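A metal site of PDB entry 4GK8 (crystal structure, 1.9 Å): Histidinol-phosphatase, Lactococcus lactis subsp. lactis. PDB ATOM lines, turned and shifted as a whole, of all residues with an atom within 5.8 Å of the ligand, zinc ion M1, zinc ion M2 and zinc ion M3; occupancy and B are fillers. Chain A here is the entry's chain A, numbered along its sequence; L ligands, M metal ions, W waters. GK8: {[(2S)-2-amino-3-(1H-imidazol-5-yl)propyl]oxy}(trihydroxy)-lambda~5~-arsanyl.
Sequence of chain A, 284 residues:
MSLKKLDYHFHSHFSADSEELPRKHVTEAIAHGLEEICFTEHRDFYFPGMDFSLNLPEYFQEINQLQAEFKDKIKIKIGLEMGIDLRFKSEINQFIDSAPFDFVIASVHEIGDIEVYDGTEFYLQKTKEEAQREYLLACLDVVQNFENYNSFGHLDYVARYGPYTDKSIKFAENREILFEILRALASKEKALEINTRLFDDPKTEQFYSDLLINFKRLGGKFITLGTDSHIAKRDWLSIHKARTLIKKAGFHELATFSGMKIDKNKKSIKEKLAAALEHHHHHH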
ATOM      1  N   HIS A   9     -11.542  16.496  33.144  1.00  0.00           N
ATOM      2  CA  HIS A   9     -11.861  16.495  31.717  1.00  0.00           C
ATOM      3  C   HIS A   9     -11.506  15.135  31.123  1.00  0.00           C
ATOM      4  O   HIS A   9     -10.336  14.826  30.945  1.00  0.00           O
ATOM      5  CB  HIS A   9     -11.094  17.607  30.979  1.00  0.00           C
ATOM      6  CG  HIS A   9     -11.528  17.819  29.557  1.00  0.00           C
ATOM      7  ND1 HIS A   9     -11.353  19.014  28.900  1.00  0.00           N
ATOM      8  CD2 HIS A   9     -12.149  16.991  28.673  1.00  0.00           C
ATOM      9  CE1 HIS A   9     -11.827  18.906  27.665  1.00  0.00           C
ATOM     10  NE2 HIS A   9     -12.322  17.692  27.508  1.00  0.00           N
ATOM     11  N   PHE A  10     -12.524  14.331  30.831  1.00  0.00           N
ATOM     12  CA  PHE A  10     -12.295  13.037  30.173  1.00  0.00           C
ATOM     13  C   PHE A  10     -13.604  12.466  29.652  1.00  0.00           C
ATOM     14  O   PHE A  10     -14.698  12.928  30.018  1.00  0.00           O
ATOM     15  CB  PHE A  10     -11.539  12.042  31.092  1.00  0.00           C
ATOM     16  CG  PHE A  10     -12.263  11.711  32.374  1.00  0.00           C
ATOM     17  CD1 PHE A  10     -13.118  10.614  32.442  1.00  0.00           C
ATOM     18  CD2 PHE A  10     -12.059  12.472  33.516  1.00  0.00           C
ATOM     19  CE1 PHE A  10     -13.783  10.301  33.616  1.00  0.00           C
ATOM     20  CE2 PHE A  10     -12.716  12.170  34.686  1.00  0.00           C
ATOM     21  CZ  PHE A  10     -13.585  11.078  34.741  1.00  0.00           C
ATOM     22  N   HIS A  11     -13.494  11.469  28.774  1.00  0.00           N
ATOM     23  CA  HIS A  11     -14.625  10.997  27.982  1.00  0.00           C
ATOM     24  C   HIS A  11     -14.753   9.484  28.000  1.00  0.00           C
ATOM     25  O   HIS A  11     -13.739   8.774  28.008  1.00  0.00           O
ATOM     26  CB  HIS A  11     -14.433  11.440  26.537  1.00  0.00           C
ATOM     27  CG  HIS A  11     -14.315  12.926  26.377  1.00  0.00           C
ATOM     28  ND1 HIS A  11     -15.400  13.728  26.110  1.00  0.00           N
ATOM     29  CD2 HIS A  11     -13.250  13.753  26.453  1.00  0.00           C
ATOM     30  CE1 HIS A  11     -15.016  14.982  26.017  1.00  0.00           C
ATOM     31  NE2 HIS A  11     -13.711  15.030  26.227  1.00  0.00           N
ATOM     32  N   SER A  15     -19.660   9.661  24.988  1.00  0.00           N
ATOM     33  CA  SER A  15     -19.224  10.657  24.006  1.00  0.00           C
ATOM     34  C   SER A  15     -19.095  10.027  22.637  1.00  0.00           C
ATOM     35  O   SER A  15     -18.699   8.864  22.530  1.00  0.00           O
ATOM     36  CB  SER A  15     -17.858  11.244  24.389  1.00  0.00           C
ATOM     37  OG  SER A  15     -17.946  12.080  25.534  1.00  0.00           O
ATOM     38  N   ASP A  17     -16.942  10.306  20.317  1.00  0.00           N
ATOM     39  CA  ASP A  17     -15.609   9.959  19.840  1.00  0.00           C
ATOM     40  C   ASP A  17     -14.800   9.147  20.862  1.00  0.00           C
ATOM     41  O   ASP A  17     -13.573   9.137  20.817  1.00  0.00           O
ATOM     42  CB  ASP A  17     -14.824  11.207  19.428  1.00  0.00           C
ATOM     43  CG  ASP A  17     -14.539  12.143  20.587  1.00  0.00           C
ATOM     44  OD1 ASP A  17     -15.134  11.951  21.657  1.00  0.00           O
ATOM     45  OD2 ASP A  17     -13.724  13.107  20.424  1.00  0.00           O
ATOM     46  N   THR A  40     -16.776  14.380  31.658  1.00  0.00           N
ATOM     47  CA  THR A  40     -17.177  15.566  30.909  1.00  0.00           C
ATOM     48  C   THR A  40     -17.476  15.188  29.463  1.00  0.00           C
ATOM     49  O   THR A  40     -16.703  15.497  28.560  1.00  0.00           O
ATOM     50  CB  THR A  40     -16.100  16.693  30.933  1.00  0.00           C
ATOM     51  OG1 THR A  40     -14.876  16.209  30.392  1.00  0.00           O
ATOM     52  CG2 THR A  40     -15.846  17.206  32.365  1.00  0.00           C
ATOM     53  N   HIS A  42     -19.084  14.787  25.636  1.00  0.00           N
ATOM     54  CA  HIS A  42     -19.368  15.758  24.561  1.00  0.00           C
ATOM     55  C   HIS A  42     -20.840  16.010  24.298  1.00  0.00           C
ATOM     56  O   HIS A  42     -21.618  15.052  24.104  1.00  0.00           O
ATOM     57  CB  HIS A  42     -18.814  15.226  23.227  1.00  0.00           C
ATOM     58  CG  HIS A  42     -17.325  15.350  23.069  1.00  0.00           C
ATOM     59  ND1 HIS A  42     -16.672  16.567  23.127  1.00  0.00           N
ATOM     60  CD2 HIS A  42     -16.383  14.422  22.793  1.00  0.00           C
ATOM     61  CE1 HIS A  42     -15.387  16.372  22.916  1.00  0.00           C
ATOM     62  NE2 HIS A  42     -15.187  15.085  22.708  1.00  0.00           N
ATOM     63  N   ASP A  44     -22.130  18.734  21.188  1.00  0.00           N
ATOM     64  CA  ASP A  44     -21.906  19.814  20.217  1.00  0.00           C
ATOM     65  C   ASP A  44     -23.122  19.812  19.276  1.00  0.00           C
ATOM     66  O   ASP A  44     -23.439  18.773  18.708  1.00  0.00           O
ATOM     67  CB  ASP A  44     -20.652  19.546  19.358  1.00  0.00           C
ATOM     68  CG  ASP A  44     -19.345  19.536  20.173  1.00  0.00           C
ATOM     69  OD1 ASP A  44     -19.068  18.514  20.852  1.00  0.00           O
ATOM     70  OD2 ASP A  44     -18.573  20.518  20.099  1.00  0.00           O
ATOM     71  N   PHE A  47     -22.992  19.558  14.637  1.00  0.00           N
ATOM     72  CA  PHE A  47     -21.562  19.498  14.384  1.00  0.00           C
ATOM     73  C   PHE A  47     -21.290  19.047  12.965  1.00  0.00           C
ATOM     74  O   PHE A  47     -21.979  18.166  12.467  1.00  0.00           O
ATOM     75  CB  PHE A  47     -20.846  18.562  15.361  1.00  0.00           C
ATOM     76  CG  PHE A  47     -19.369  18.828  15.488  1.00  0.00           C
ATOM     77  CD1 PHE A  47     -18.929  19.947  16.190  1.00  0.00           C
ATOM     78  CD2 PHE A  47     -18.437  18.010  14.876  1.00  0.00           C
ATOM     79  CE1 PHE A  47     -17.573  20.217  16.314  1.00  0.00           C
ATOM     80  CE2 PHE A  47     -17.074  18.272  14.990  1.00  0.00           C
ATOM     81  CZ  PHE A  47     -16.642  19.376  15.709  1.00  0.00           C
ATOM     82  N   MET A  50     -20.092  14.833  11.843  1.00  0.00           N
ATOM     83  CA  MET A  50     -20.236  13.804  12.859  1.00  0.00           C
ATOM     84  C   MET A  50     -21.111  14.296  14.003  1.00  0.00           C
ATOM     85  O   MET A  50     -20.927  15.404  14.500  1.00  0.00           O
ATOM     86  CB  MET A  50     -18.852  13.441  13.394  1.00  0.00           C
ATOM     87  CG  MET A  50     -18.850  12.447  14.543  1.00  0.00           C
ATOM     88  SD  MET A  50     -17.142  12.146  15.037  1.00  0.00           S
ATOM     89  CE  MET A  50     -17.399  11.053  16.422  1.00  0.00           C
ATOM     90  N   PHE A  52     -22.367  14.783  17.626  1.00  0.00           N
ATOM     91  CA  PHE A  52     -21.945  14.688  19.019  1.00  0.00           C
ATOM     92  C   PHE A  52     -23.150  14.849  19.930  1.00  0.00           C
ATOM     93  O   PHE A  52     -23.371  15.896  20.530  1.00  0.00           O
ATOM     94  CB  PHE A  52     -20.859  15.738  19.345  1.00  0.00           C
ATOM     95  CG  PHE A  52     -19.486  15.336  18.893  1.00  0.00           C
ATOM     96  CD1 PHE A  52     -18.632  14.656  19.749  1.00  0.00           C
ATOM     97  CD2 PHE A  52     -19.058  15.615  17.611  1.00  0.00           C
ATOM     98  CE1 PHE A  52     -17.368  14.284  19.340  1.00  0.00           C
ATOM     99  CE2 PHE A  52     -17.780  15.242  17.201  1.00  0.00           C
ATOM    100  CZ  PHE A  52     -16.940  14.573  18.060  1.00  0.00           C
ATOM    101  N   GLU A  81     -18.701  18.535  28.496  1.00  0.00           N
ATOM    102  CA  GLU A  81     -17.913  19.417  27.645  1.00  0.00           C
ATOM    103  C   GLU A  81     -18.813  19.918  26.539  1.00  0.00           C
ATOM    104  O   GLU A  81     -19.165  19.176  25.623  1.00  0.00           O
ATOM    105  CB  GLU A  81     -16.660  18.743  27.063  1.00  0.00           C
ATOM    106  CG  GLU A  81     -15.820  19.761  26.263  1.00  0.00           C
ATOM    107  CD  GLU A  81     -14.665  19.154  25.475  1.00  0.00           C
ATOM    108  OE1 GLU A  81     -14.507  17.923  25.434  1.00  0.00           O
ATOM    109  OE2 GLU A  81     -13.898  19.955  24.881  1.00  0.00           O
ATOM    110  N   SER A 107     -16.062  24.979  25.207  1.00  0.00           N
ATOM    111  CA  SER A 107     -14.974  24.722  24.275  1.00  0.00           C
ATOM    112  C   SER A 107     -15.357  25.221  22.893  1.00  0.00           C
ATOM    113  O   SER A 107     -16.536  25.238  22.538  1.00  0.00           O
ATOM    114  CB  SER A 107     -14.726  23.218  24.165  1.00  0.00           C
ATOM    115  OG  SER A 107     -14.136  22.696  25.348  1.00  0.00           O
ATOM    116  N   HIS A 109     -14.816  24.075  19.076  1.00  0.00           N
ATOM    117  CA  HIS A 109     -14.426  22.918  18.265  1.00  0.00           C
ATOM    118  C   HIS A 109     -14.656  23.139  16.774  1.00  0.00           C
ATOM    119  O   HIS A 109     -14.105  22.432  15.919  1.00  0.00           O
ATOM    120  CB  HIS A 109     -15.209  21.675  18.693  1.00  0.00           C
ATOM    121  CG  HIS A 109     -14.869  21.184  20.064  1.00  0.00           C
ATOM    122  ND1 HIS A 109     -15.821  20.724  20.945  1.00  0.00           N
ATOM    123  CD2 HIS A 109     -13.675  21.073  20.708  1.00  0.00           C
ATOM    124  CE1 HIS A 109     -15.235  20.357  22.074  1.00  0.00           C
ATOM    125  NE2 HIS A 109     -13.935  20.552  21.959  1.00  0.00           N
ATOM    126  N   GLU A 115     -14.897  22.398  10.990  1.00  0.00           N
ATOM    127  CA  GLU A 115     -14.277  21.819  12.176  1.00  0.00           C
ATOM    128  C   GLU A 115     -12.786  22.161  12.290  1.00  0.00           C
ATOM    129  O   GLU A 115     -12.044  22.118  11.310  1.00  0.00           O
ATOM    130  CB  GLU A 115     -14.457  20.290  12.196  1.00  0.00           C
ATOM    131  CG  GLU A 115     -13.800  19.646  13.404  1.00  0.00           C
ATOM    132  CD  GLU A 115     -13.928  18.133  13.422  1.00  0.00           C
ATOM    133  OE1 GLU A 115     -14.287  17.544  12.392  1.00  0.00           O
ATOM    134  OE2 GLU A 115     -13.665  17.548  14.488  1.00  0.00           O
ATOM    135  N   VAL A 116     -12.361  22.529  13.491  1.00  0.00           N
ATOM    136  CA  VAL A 116     -10.944  22.732  13.770  1.00  0.00           C
ATOM    137  C   VAL A 116     -10.352  21.357  14.088  1.00  0.00           C
ATOM    138  O   VAL A 116     -10.521  20.842  15.189  1.00  0.00           O
ATOM    139  CB  VAL A 116     -10.746  23.712  14.954  1.00  0.00           C
ATOM    140  CG1 VAL A 116      -9.248  23.966  15.211  1.00  0.00           C
ATOM    141  CG2 VAL A 116     -11.485  25.017  14.678  1.00  0.00           C
ATOM    142  N   TYR A 117      -9.677  20.747  13.119  1.00  0.00           N
ATOM    143  CA  TYR A 117      -9.222  19.376  13.278  1.00  0.00           C
ATOM    144  C   TYR A 117      -8.291  19.021  12.147  1.00  0.00           C
ATOM    145  O   TYR A 117      -8.207  19.756  11.179  1.00  0.00           O
ATOM    146  CB  TYR A 117     -10.409  18.407  13.293  1.00  0.00           C
ATOM    147  CG  TYR A 117     -10.101  17.099  13.997  1.00  0.00           C
ATOM    148  CD1 TYR A 117      -9.988  17.051  15.384  1.00  0.00           C
ATOM    149  CD2 TYR A 117      -9.943  15.917  13.281  1.00  0.00           C
ATOM    150  CE1 TYR A 117      -9.706  15.865  16.047  1.00  0.00           C
ATOM    151  CE2 TYR A 117      -9.662  14.721  13.940  1.00  0.00           C
ATOM    152  CZ  TYR A 117      -9.539  14.708  15.316  1.00  0.00           C
ATOM    153  OH  TYR A 117      -9.270  13.533  15.982  1.00  0.00           O
ATOM    154  N   HIS A 154      -9.336  23.953  26.895  1.00  0.00           N
ATOM    155  CA  HIS A 154      -8.175  23.930  25.999  1.00  0.00           C
ATOM    156  C   HIS A 154      -7.960  25.127  25.059  1.00  0.00           C
ATOM    157  O   HIS A 154      -8.284  25.068  23.881  1.00  0.00           O
ATOM    158  CB  HIS A 154      -8.142  22.602  25.187  1.00  0.00           C
ATOM    159  CG  HIS A 154      -9.440  22.249  24.513  1.00  0.00           C
ATOM    160  ND1 HIS A 154     -10.174  23.145  23.762  1.00  0.00           N
ATOM    161  CD2 HIS A 154     -10.122  21.084  24.466  1.00  0.00           C
ATOM    162  CE1 HIS A 154     -11.250  22.537  23.274  1.00  0.00           C
ATOM    163  NE2 HIS A 154     -11.245  21.285  23.685  1.00  0.00           N
ATOM    164  N   TYR A 157      -6.126  24.324  21.852  1.00  0.00           N
ATOM    165  CA  TYR A 157      -6.743  23.309  20.989  1.00  0.00           C
ATOM    166  C   TYR A 157      -6.258  23.393  19.538  1.00  0.00           C
ATOM    167  O   TYR A 157      -5.973  22.374  18.893  1.00  0.00           O
ATOM    168  CB  TYR A 157      -8.271  23.442  21.053  1.00  0.00           C
ATOM    169  CG  TYR A 157      -9.083  22.365  20.353  1.00  0.00           C
ATOM    170  CD1 TYR A 157      -9.308  21.129  20.954  1.00  0.00           C
ATOM    171  CD2 TYR A 157      -9.693  22.620  19.122  1.00  0.00           C
ATOM    172  CE1 TYR A 157     -10.084  20.162  20.327  1.00  0.00           C
ATOM    173  CE2 TYR A 157     -10.463  21.654  18.487  1.00  0.00           C
ATOM    174  CZ  TYR A 157     -10.650  20.432  19.099  1.00  0.00           C
ATOM    175  OH  TYR A 157     -11.411  19.474  18.473  1.00  0.00           O
ATOM    176  N   ARG A 160      -3.152  21.528  18.390  1.00  0.00           N
ATOM    177  CA  ARG A 160      -3.111  20.076  18.288  1.00  0.00           C
ATOM    178  C   ARG A 160      -3.033  19.626  16.838  1.00  0.00           C
ATOM    179  O   ARG A 160      -2.534  18.540  16.553  1.00  0.00           O
ATOM    180  CB  ARG A 160      -4.337  19.440  18.927  1.00  0.00           C
ATOM    181  CG  ARG A 160      -4.513  19.730  20.417  1.00  0.00           C
ATOM    182  CD  ARG A 160      -5.888  19.222  20.841  1.00  0.00           C
ATOM    183  NE  ARG A 160      -6.100  19.320  22.284  1.00  0.00           N
ATOM    184  CZ  ARG A 160      -7.129  18.743  22.899  1.00  0.00           C
ATOM    185  NH1 ARG A 160      -7.993  18.040  22.174  1.00  0.00           N
ATOM    186  NH2 ARG A 160      -7.269  18.852  24.218  1.00  0.00           N
ATOM    187  N   TYR A 161      -3.551  20.433  15.925  1.00  0.00           N
ATOM    188  CA  TYR A 161      -3.870  19.928  14.587  1.00  0.00           C
ATOM    189  C   TYR A 161      -3.315  20.827  13.503  1.00  0.00           C
ATOM    190  O   TYR A 161      -2.819  21.909  13.774  1.00  0.00           O
ATOM    191  CB  TYR A 161      -5.389  19.781  14.403  1.00  0.00           C
ATOM    192  CG  TYR A 161      -6.104  19.163  15.591  1.00  0.00           C
ATOM    193  CD1 TYR A 161      -5.960  17.808  15.875  1.00  0.00           C
ATOM    194  CD2 TYR A 161      -6.913  19.938  16.423  1.00  0.00           C
ATOM    195  CE1 TYR A 161      -6.611  17.231  16.977  1.00  0.00           C
ATOM    196  CE2 TYR A 161      -7.557  19.372  17.522  1.00  0.00           C
ATOM    197  CZ  TYR A 161      -7.406  18.023  17.785  1.00  0.00           C
ATOM    198  OH  TYR A 161      -8.043  17.459  18.877  1.00  0.00           O
ATOM    199  N   ASN A 195      -5.204  21.966  30.320  1.00  0.00           N
ATOM    200  CA  ASN A 195      -5.485  20.732  29.592  1.00  0.00           C
ATOM    201  C   ASN A 195      -4.168  20.043  29.264  1.00  0.00           C
ATOM    202  O   ASN A 195      -3.311  20.630  28.613  1.00  0.00           O
ATOM    203  CB  ASN A 195      -6.261  21.077  28.305  1.00  0.00           C
ATOM    204  CG  ASN A 195      -6.797  19.843  27.599  1.00  0.00           C
ATOM    205  OD1 ASN A 195      -6.050  18.925  27.265  1.00  0.00           O
ATOM    206  ND2 ASN A 195      -8.100  19.823  27.369  1.00  0.00           N
ATOM    207  N   ARG A 197      -3.354  17.445  27.362  1.00  0.00           N
ATOM    208  CA  ARG A 197      -3.237  16.666  26.131  1.00  0.00           C
ATOM    209  C   ARG A 197      -1.844  16.748  25.479  1.00  0.00           C
ATOM    210  O   ARG A 197      -1.241  15.715  25.193  1.00  0.00           O
ATOM    211  CB  ARG A 197      -4.321  17.042  25.116  1.00  0.00           C
ATOM    212  CG  ARG A 197      -4.102  16.387  23.729  1.00  0.00           C
ATOM    213  CD  ARG A 197      -4.346  14.874  23.720  1.00  0.00           C
ATOM    214  NE  ARG A 197      -5.737  14.555  24.056  1.00  0.00           N
ATOM    215  CZ  ARG A 197      -6.763  14.690  23.214  1.00  0.00           C
ATOM    216  NH1 ARG A 197      -6.566  15.127  21.982  1.00  0.00           N
ATOM    217  NH2 ARG A 197      -7.997  14.403  23.624  1.00  0.00           N
ATOM    218  N   ASP A 228      -8.154  15.229  29.282  1.00  0.00           N
ATOM    219  CA  ASP A 228      -8.845  15.043  28.006  1.00  0.00           C
ATOM    220  C   ASP A 228      -8.714  13.603  27.475  1.00  0.00           C
ATOM    221  O   ASP A 228      -8.751  13.372  26.270  1.00  0.00           O
ATOM    222  CB  ASP A 228      -8.357  16.036  26.947  1.00  0.00           C
ATOM    223  CG  ASP A 228      -9.490  16.564  26.072  1.00  0.00           C
ATOM    224  OD1 ASP A 228     -10.565  15.928  25.999  1.00  0.00           O
ATOM    225  OD2 ASP A 228      -9.297  17.626  25.460  1.00  0.00           O
ATOM    226  N   HIS A 230      -9.572   9.959  26.298  1.00  0.00           N
ATOM    227  CA  HIS A 230     -10.710   9.271  25.720  1.00  0.00           C
ATOM    228  C   HIS A 230     -10.589   7.768  25.979  1.00  0.00           C
ATOM    229  O   HIS A 230     -11.472   6.999  25.627  1.00  0.00           O
ATOM    230  CB  HIS A 230     -10.827   9.564  24.226  1.00  0.00           C
ATOM    231  CG  HIS A 230     -11.235  10.982  23.940  1.00  0.00           C
ATOM    232  ND1 HIS A 230     -10.548  12.065  24.437  1.00  0.00           N
ATOM    233  CD2 HIS A 230     -12.262  11.480  23.216  1.00  0.00           C
ATOM    234  CE1 HIS A 230     -11.136  13.173  24.025  1.00  0.00           C
ATOM    235  NE2 HIS A 230     -12.179  12.846  23.279  1.00  0.00           N
HETATM  236  C   GK8 L   1     -12.152  16.143  19.858  1.00  0.00           C
HETATM  237  N   GK8 L   1     -13.934  17.756  19.614  1.00  0.00           N
HETATM  238 AS   GK8 L   1     -11.741  16.718  22.518  1.00  0.00          AS
HETATM  239  O1  GK8 L   1      -9.978  16.659  22.472  1.00  0.00           O
HETATM  240  O2  GK8 L   1     -12.444  18.291  22.052  1.00  0.00           O
HETATM  241  O3  GK8 L   1     -12.535  16.025  23.936  1.00  0.00           O
HETATM  242  O4  GK8 L   1     -12.215  15.649  21.149  1.00  0.00           O
HETATM  243  CA  GK8 L   1     -13.441  16.484  19.157  1.00  0.00           C
HETATM  244  CB  GK8 L   1     -13.269  16.533  17.665  1.00  0.00           C
HETATM  245  CG  GK8 L   1     -13.336  15.260  16.881  1.00  0.00           C
HETATM  246  ND1 GK8 L   1     -13.597  15.137  15.554  1.00  0.00           N
HETATM  247  CD2 GK8 L   1     -13.147  13.964  17.362  1.00  0.00           C
HETATM  248  CE1 GK8 L   1     -13.569  13.845  15.222  1.00  0.00           C
HETATM  249  NE2 GK8 L   1     -13.294  13.134  16.315  1.00  0.00           N
HETATM  250 ZN    ZN M   1     -12.613  16.785  25.606  1.00  0.00          ZN
HETATM  251 ZN    ZN M   2     -12.645  19.712  23.354  1.00  0.00          ZN
HETATM  252 ZN    ZN M   3     -13.391  14.170  22.189  1.00  0.00          ZN
HETATM  253  O   HOH W   1     -16.511  17.654  19.631  1.00  0.00           O
HETATM  254  O   HOH W   2     -11.687  18.386  24.606  1.00  0.00           O
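OH of Tyr 157 lies within hydrogen-bond range of N of the ligand (3.3 Å).
The guanidinium group of Arg 197 is in hydrogen-bond range of an oxygen (O1) of the ligand.
O1 of the ligand is in hydrogen-bond range of NH1 of Arg 160, 2.4 Å away.
A nitrogen (ND1) of the ligand lies within hydrogen-bond range of the side-chain carboxylate of Glu 115 (2.6 Å).
Of the 25 residues printed, 3 come within 4 Å of zinc ion M3.
Along chain A the residues within 4 Å of zinc ion M3 span positions 17 to 230.
An oxygen (O3) of the ligand is bound to zinc ion M1, at 1.8 Å.
Water W2 is bound to zinc ion M1, 2.1 Å away.
NE2 of His 9 is bound to zinc ion M1, at 2.1 Å.
NE2 of His 11 binds zinc ion M1 (2.2 Å).
Zinc ion M1 is bound by OE1 of Glu 81 (2.2 Å).
The side-chain carboxylate (OD1) of Asp 228 binds zinc ion M1 (2.3 Å).
Zinc ion M1 has six donor atoms within binding distance.
Residues that only touch the ligand: Tyr 117, Phe 52 and Met 50.
Hydrophobic or aromatic side chains within 4 Å of the ligand: His 11, His 42, Met 50, Phe 52, His 109, Tyr 117, Tyr 157 and His 230.
16 residues have an atom within 4 Å of the ligand: His 9, His 11, Asp 17, His 42, Met 50, Phe 52, Glu 81, His 109, Glu 115, Tyr 117, His 154, Tyr 157, Arg 160, Arg 197, Asp 228 and His 230.
Ser 107 touches zinc ion M2 (OG to ZN, 3.9 Å).
CE1 of Tyr 157 touches zinc ion M2, 3.99 Å away.
Five residues have an atom within 4 Å of zinc ion M2: Glu 81, Ser 107, His 109, His 154 and Tyr 157.
Along chain A the residues within 4 Å of zinc ion M2 span positions 81 to 157.
The nearest printed residue that does not touch zinc ion M2 is His 42 (4.3 Å).
Water W2 bridges the side-chain carboxylate of Asp 228 (2.6 Å) and an oxygen (O1) of the ligand (3.2 Å).
Water W1 lies within hydrogen-bond range of a nitrogen (N) of the ligand, the side-chain carboxylate (OD1) of Asp 44 and a ring nitrogen (ND1) of His 109.
Zinc ion M2 is bound by O2 of the ligand, OE2 of Glu 81, water W2, NE2 of His 109 and NE2 of His 154.
Of the 25 residues printed, 5 come within 4 Å of zinc ion M1.
The side-chain carboxylate of Glu 81 sits close to a ring nitrogen (ND1) of His 42, 3.4 Å away.
The guanidinium group (NH2) of Arg 197 lies within salt-bridge range of the side-chain carboxylate (OD2) of Asp 228, at 3.9 Å.
O of Thr 40 lies close to ND1 of His 11, 3.3 Å away.
The backbone NH (N) of Val 116 is in hydrogen-bond range of the backbone carbonyl oxygen (O) of His 109.
The backbone carbonyl oxygen of Phe 52 sits at hydrogen-bond distance from the backbone NH of Asp 44 (3.2 Å).
OD2 of Asp 228 is in salt-bridge range of NH2 of Arg 160.
The guanidinium group (NH1) of Arg 160 is in hydrogen-bond range of the side-chain hydroxyl (OH) of Tyr 161, at 3.3 Å.
A ring nitrogen (ND1) of His 11 lies within hydrogen-bond range of the side-chain hydroxyl (OG) of Ser 15, at 3.1 Å.
Zinc ion M3 is bound by a ring nitrogen (NE2) of His 42, the side-chain carboxylate (OD2) of Asp 17, a ring nitrogen (NE2) of His 230 and an oxygen (O4) of the ligand.
Zinc ion M3 has four donor atoms within binding distance.
Slightly farther from zinc ion M3 lies an oxygen (O3) of the ligand (2.7 Å).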
